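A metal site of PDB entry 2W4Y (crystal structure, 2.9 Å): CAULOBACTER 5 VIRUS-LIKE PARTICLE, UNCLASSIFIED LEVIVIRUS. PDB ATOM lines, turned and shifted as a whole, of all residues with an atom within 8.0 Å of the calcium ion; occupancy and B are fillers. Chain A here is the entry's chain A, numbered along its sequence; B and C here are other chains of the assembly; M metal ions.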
ATOM      1  N   ASN A  24       7.637  15.349 -22.610  1.00  0.00           N
ATOM      2  CA  ASN A  24       8.052  14.460 -21.542  1.00  0.00           C
ATOM      3  C   ASN A  24       9.268  13.623 -21.912  1.00  0.00           C
ATOM      4  O   ASN A  24       9.468  13.294 -23.076  1.00  0.00           O
ATOM      5  CB  ASN A  24       6.893  13.558 -21.143  1.00  0.00           C
ATOM      6  CG  ASN A  24       7.132  12.842 -19.837  1.00  0.00           C
ATOM      7  OD1 ASN A  24       7.358  13.480 -18.794  1.00  0.00           O
ATOM      8  ND2 ASN A  24       7.081  11.521 -19.874  1.00  0.00           N
ATOM      9  N   GLN A  25      10.087  13.287 -20.917  1.00  0.00           N
ATOM     10  CA  GLN A  25      11.258  12.459 -21.168  1.00  0.00           C
ATOM     11  C   GLN A  25      11.525  11.677 -19.900  1.00  0.00           C
ATOM     12  O   GLN A  25      11.872  12.240 -18.866  1.00  0.00           O
ATOM     13  CB  GLN A  25      12.458  13.327 -21.595  1.00  0.00           C
ATOM     14  CG  GLN A  25      13.612  13.421 -20.606  1.00  0.00           C
ATOM     15  CD  GLN A  25      14.451  12.157 -20.516  1.00  0.00           C
ATOM     16  OE1 GLN A  25      15.407  12.102 -19.742  1.00  0.00           O
ATOM     17  NE2 GLN A  25      14.112  11.141 -21.292  1.00  0.00           N
ATOM     18  N   ASP A  26      11.325  10.366 -20.001  1.00  0.00           N
ATOM     19  CA  ASP A  26      11.515   9.441 -18.879  1.00  0.00           C
ATOM     20  C   ASP A  26      12.078   8.133 -19.435  1.00  0.00           C
ATOM     21  O   ASP A  26      11.757   7.749 -20.557  1.00  0.00           O
ATOM     22  CB  ASP A  26      10.166   9.146 -18.220  1.00  0.00           C
ATOM     23  CG  ASP A  26       9.633  10.315 -17.399  1.00  0.00           C
ATOM     24  OD1 ASP A  26       8.391  10.429 -17.271  1.00  0.00           O
ATOM     25  OD2 ASP A  26      10.470  11.101 -16.865  1.00  0.00           O
ATOM     26  N   GLY A  27      12.908   7.463 -18.638  1.00  0.00           N
ATOM     27  CA  GLY A  27      13.487   6.193 -19.039  1.00  0.00           C
ATOM     28  C   GLY A  27      14.165   6.106 -20.391  1.00  0.00           C
ATOM     29  O   GLY A  27      13.907   5.182 -21.150  1.00  0.00           O
ATOM     30  N   TYR A  28      15.047   7.058 -20.701  1.00  0.00           N
ATOM     31  CA  TYR A  28      15.745   7.040 -21.982  1.00  0.00           C
ATOM     32  C   TYR A  28      14.704   7.056 -23.096  1.00  0.00           C
ATOM     33  O   TYR A  28      14.783   6.304 -24.061  1.00  0.00           O
ATOM     34  CB  TYR A  28      16.610   5.795 -22.104  1.00  0.00           C
ATOM     35  CG  TYR A  28      17.517   5.599 -20.905  1.00  0.00           C
ATOM     36  CD1 TYR A  28      17.115   4.823 -19.829  1.00  0.00           C
ATOM     37  CD2 TYR A  28      18.756   6.241 -20.822  1.00  0.00           C
ATOM     38  CE1 TYR A  28      17.924   4.670 -18.716  1.00  0.00           C
ATOM     39  CE2 TYR A  28      19.577   6.106 -19.714  1.00  0.00           C
ATOM     40  CZ  TYR A  28      19.151   5.314 -18.660  1.00  0.00           C
ATOM     41  OH  TYR A  28      19.959   5.154 -17.555  1.00  0.00           O
ATOM     42  N   THR A  29      13.741   7.955 -22.931  1.00  0.00           N
ATOM     43  CA  THR A  29      12.637   8.100 -23.844  1.00  0.00           C
ATOM     44  C   THR A  29      12.224   9.542 -23.962  1.00  0.00           C
ATOM     45  O   THR A  29      12.369  10.311 -23.020  1.00  0.00           O
ATOM     46  CB  THR A  29      11.432   7.287 -23.333  1.00  0.00           C
ATOM     47  OG1 THR A  29      11.615   5.922 -23.664  1.00  0.00           O
ATOM     48  CG2 THR A  29      10.122   7.806 -23.906  1.00  0.00           C
ATOM     49  N   ASN B  24      19.324  11.382 -20.232  1.00  0.00           N
ATOM     50  CA  ASN B  24      18.203  11.000 -19.389  1.00  0.00           C
ATOM     51  C   ASN B  24      18.170  11.803 -18.093  1.00  0.00           C
ATOM     52  O   ASN B  24      19.193  12.271 -17.608  1.00  0.00           O
ATOM     53  CB  ASN B  24      18.238   9.509 -19.069  1.00  0.00           C
ATOM     54  CG  ASN B  24      16.930   9.010 -18.485  1.00  0.00           C
ATOM     55  OD1 ASN B  24      15.865   9.142 -19.102  1.00  0.00           O
ATOM     56  ND2 ASN B  24      17.000   8.438 -17.285  1.00  0.00           N
ATOM     57  N   GLN B  25      16.973  11.984 -17.551  1.00  0.00           N
ATOM     58  CA  GLN B  25      16.794  12.700 -16.311  1.00  0.00           C
ATOM     59  C   GLN B  25      15.501  12.258 -15.658  1.00  0.00           C
ATOM     60  O   GLN B  25      14.409  12.600 -16.111  1.00  0.00           O
ATOM     61  CB  GLN B  25      16.827  14.219 -16.554  1.00  0.00           C
ATOM     62  CG  GLN B  25      15.660  15.031 -15.959  1.00  0.00           C
ATOM     63  CD  GLN B  25      15.520  14.912 -14.450  1.00  0.00           C
ATOM     64  OE1 GLN B  25      14.482  15.259 -13.898  1.00  0.00           O
ATOM     65  NE2 GLN B  25      16.569  14.440 -13.774  1.00  0.00           N
ATOM     66  N   ASP B  26      15.645  11.466 -14.601  1.00  0.00           N
ATOM     67  CA  ASP B  26      14.520  10.938 -13.855  1.00  0.00           C
ATOM     68  C   ASP B  26      14.831  10.960 -12.368  1.00  0.00           C
ATOM     69  O   ASP B  26      15.961  10.740 -11.962  1.00  0.00           O
ATOM     70  CB  ASP B  26      14.273   9.485 -14.258  1.00  0.00           C
ATOM     71  CG  ASP B  26      13.734   9.346 -15.671  1.00  0.00           C
ATOM     72  OD1 ASP B  26      14.005   8.284 -16.280  1.00  0.00           O
ATOM     73  OD2 ASP B  26      13.036  10.273 -16.158  1.00  0.00           O
ATOM     74  N   GLY B  27      13.807  11.234 -11.571  1.00  0.00           N
ATOM     75  CA  GLY B  27      13.972  11.263 -10.132  1.00  0.00           C
ATOM     76  C   GLY B  27      15.161  12.022  -9.576  1.00  0.00           C
ATOM     77  O   GLY B  27      15.919  11.477  -8.793  1.00  0.00           O
ATOM     78  N   TYR B  28      15.313  13.284  -9.974  1.00  0.00           N
ATOM     79  CA  TYR B  28      16.419  14.107  -9.485  1.00  0.00           C
ATOM     80  C   TYR B  28      17.713  13.411  -9.829  1.00  0.00           C
ATOM     81  O   TYR B  28      18.603  13.262  -8.989  1.00  0.00           O
ATOM     82  CB  TYR B  28      16.316  14.279  -7.977  1.00  0.00           C
ATOM     83  CG  TYR B  28      14.926  14.655  -7.530  1.00  0.00           C
ATOM     84  CD1 TYR B  28      14.061  13.695  -7.008  1.00  0.00           C
ATOM     85  CD2 TYR B  28      14.462  15.960  -7.679  1.00  0.00           C
ATOM     86  CE1 TYR B  28      12.768  14.032  -6.643  1.00  0.00           C
ATOM     87  CE2 TYR B  28      13.161  16.307  -7.310  1.00  0.00           C
ATOM     88  CZ  TYR B  28      12.318  15.338  -6.795  1.00  0.00           C
ATOM     89  OH  TYR B  28      11.039  15.682  -6.425  1.00  0.00           O
ATOM     90  N   THR B  29      17.799  12.981 -11.082  1.00  0.00           N
ATOM     91  CA  THR B  29      18.952  12.242 -11.551  1.00  0.00           C
ATOM     92  C   THR B  29      19.195  12.519 -13.012  1.00  0.00           C
ATOM     93  O   THR B  29      18.280  12.439 -13.828  1.00  0.00           O
ATOM     94  CB  THR B  29      18.702  10.729 -11.390  1.00  0.00           C
ATOM     95  OG1 THR B  29      18.982  10.345 -10.042  1.00  0.00           O
ATOM     96  CG2 THR B  29      19.533   9.913 -12.376  1.00  0.00           C
ATOM     97  N   ASN C  24      13.836  18.546 -11.672  1.00  0.00           N
ATOM     98  CA  ASN C  24      13.227  17.282 -12.068  1.00  0.00           C
ATOM     99  C   ASN C  24      12.055  17.442 -13.030  1.00  0.00           C
ATOM    100  O   ASN C  24      11.368  18.469 -13.037  1.00  0.00           O
ATOM    101  CB  ASN C  24      12.774  16.521 -10.823  1.00  0.00           C
ATOM    102  CG  ASN C  24      12.495  15.066 -11.124  1.00  0.00           C
ATOM    103  OD1 ASN C  24      13.361  14.338 -11.619  1.00  0.00           O
ATOM    104  ND2 ASN C  24      11.285  14.620 -10.818  1.00  0.00           N
ATOM    105  N   GLN C  25      11.847  16.412 -13.846  1.00  0.00           N
ATOM    106  CA  GLN C  25      10.763  16.369 -14.820  1.00  0.00           C
ATOM    107  C   GLN C  25      10.424  14.918 -15.175  1.00  0.00           C
ATOM    108  O   GLN C  25      11.159  14.241 -15.898  1.00  0.00           O
ATOM    109  CB  GLN C  25      11.116  17.219 -16.057  1.00  0.00           C
ATOM    110  CG  GLN C  25      11.039  16.541 -17.420  1.00  0.00           C
ATOM    111  CD  GLN C  25       9.667  15.993 -17.757  1.00  0.00           C
ATOM    112  OE1 GLN C  25       9.545  15.016 -18.507  1.00  0.00           O
ATOM    113  NE2 GLN C  25       8.615  16.612 -17.225  1.00  0.00           N
ATOM    114  N   ASP C  26       9.307  14.440 -14.641  1.00  0.00           N
ATOM    115  CA  ASP C  26       8.845  13.091 -14.861  1.00  0.00           C
ATOM    116  C   ASP C  26       7.313  13.078 -14.930  1.00  0.00           C
ATOM    117  O   ASP C  26       6.657  13.901 -14.295  1.00  0.00           O
ATOM    118  CB  ASP C  26       9.307  12.154 -13.711  1.00  0.00           C
ATOM    119  CG  ASP C  26      10.840  12.033 -13.586  1.00  0.00           C
ATOM    120  OD1 ASP C  26      11.558  11.890 -14.615  1.00  0.00           O
ATOM    121  OD2 ASP C  26      11.313  12.011 -12.428  1.00  0.00           O
ATOM    122  N   GLY C  27       6.754  12.165 -15.713  1.00  0.00           N
ATOM    123  CA  GLY C  27       5.311  12.040 -15.823  1.00  0.00           C
ATOM    124  C   GLY C  27       4.532  13.270 -16.244  1.00  0.00           C
ATOM    125  O   GLY C  27       3.457  13.511 -15.714  1.00  0.00           O
ATOM    126  N   TYR C  28       5.051  14.052 -17.186  1.00  0.00           N
ATOM    127  CA  TYR C  28       4.377  15.273 -17.635  1.00  0.00           C
ATOM    128  C   TYR C  28       4.297  16.196 -16.419  1.00  0.00           C
ATOM    129  O   TYR C  28       3.254  16.797 -16.132  1.00  0.00           O
ATOM    130  CB  TYR C  28       2.974  14.951 -18.154  1.00  0.00           C
ATOM    131  CG  TYR C  28       2.941  13.751 -19.087  1.00  0.00           C
ATOM    132  CD1 TYR C  28       2.561  12.500 -18.624  1.00  0.00           C
ATOM    133  CD2 TYR C  28       3.311  13.881 -20.435  1.00  0.00           C
ATOM    134  CE1 TYR C  28       2.557  11.396 -19.471  1.00  0.00           C
ATOM    135  CE2 TYR C  28       3.315  12.772 -21.279  1.00  0.00           C
ATOM    136  CZ  TYR C  28       2.923  11.540 -20.792  1.00  0.00           C
ATOM    137  OH  TYR C  28       2.895  10.456 -21.642  1.00  0.00           O
ATOM    138  N   THR C  29       5.431  16.308 -15.735  1.00  0.00           N
ATOM    139  CA  THR C  29       5.539  17.115 -14.538  1.00  0.00           C
ATOM    140  C   THR C  29       6.921  17.709 -14.366  1.00  0.00           C
ATOM    141  O   THR C  29       7.924  17.020 -14.472  1.00  0.00           O
ATOM    142  CB  THR C  29       5.242  16.271 -13.310  1.00  0.00           C
ATOM    143  OG1 THR C  29       3.846  15.981 -13.283  1.00  0.00           O
ATOM    144  CG2 THR C  29       5.646  16.993 -12.032  1.00  0.00           C
HETATM  145 CA    CA M   1      12.269  12.470 -16.620  1.00  0.00          CA
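The calcium ion is bound by O of Gln 25 of chain B. OD1 of Asp 26 of chain C is bound to the calcium ion (2.2 Å). The calcium ion is bound by O of Gln 25 of chain C. The calcium ion is bound by OD2 of Asp 26 of chain A (2.3 Å). The calcium ion is bound by O of Gln 25 of chain A (2.3 Å). OD2 of Asp 26 of chain B is bound to the calcium ion, at 2.4 Å. The calcium ion has six donor atoms within binding distance.
The side-chain amide oxygen (OE1) of Gln 25 of chain A sits close to the side-chain amide oxygen (OD1) of Asn 24 of chain B, 3.1 Å away. The backbone NH (N) of Gly 27 of chain B lies within hydrogen-bond range of the side-chain carboxylate (OD2) of Asp 26 of chain C (2.7 Å). The side-chain amide oxygen of Gln 25 of chain C sits close to the side-chain amide oxygen of Asn 24 of chain A (2.7 Å). The side-chain carboxylate of Asp 26 of chain A sits at hydrogen-bond distance from the side-chain amide nitrogen of Asn 24 of chain A (3.1 Å). The backbone carbonyl oxygen (O) of Thr 29 of chain C lies within hydrogen-bond range of the side-chain amide nitrogen (NE2) of Gln 25 of chain C. OD1 of Asp 26 of chain B lies within hydrogen-bond range of N of Gly 27 of chain A. The side-chain amide nitrogen (ND2) of Asn 24 of chain B lies within hydrogen-bond range of the side-chain carboxylate (OD1) of Asp 26 of chain B, 3.2 Å away. The side-chain amide nitrogen (ND2) of Asn 24 of chain C is in hydrogen-bond range of the side-chain carboxylate (OD2) of Asp 26 of chain C (3.1 Å).
Within 4 Å of the calcium ion: Gln 25 of chain A, Asp 26 of chain A, Gln 25 of chain B, Asp 26 of chain B, Gln 25 of chain C and Asp 26 of chain C. The nearest printed residue that does not touch the calcium ion is Gly 27 of chain B (5.4 Å).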
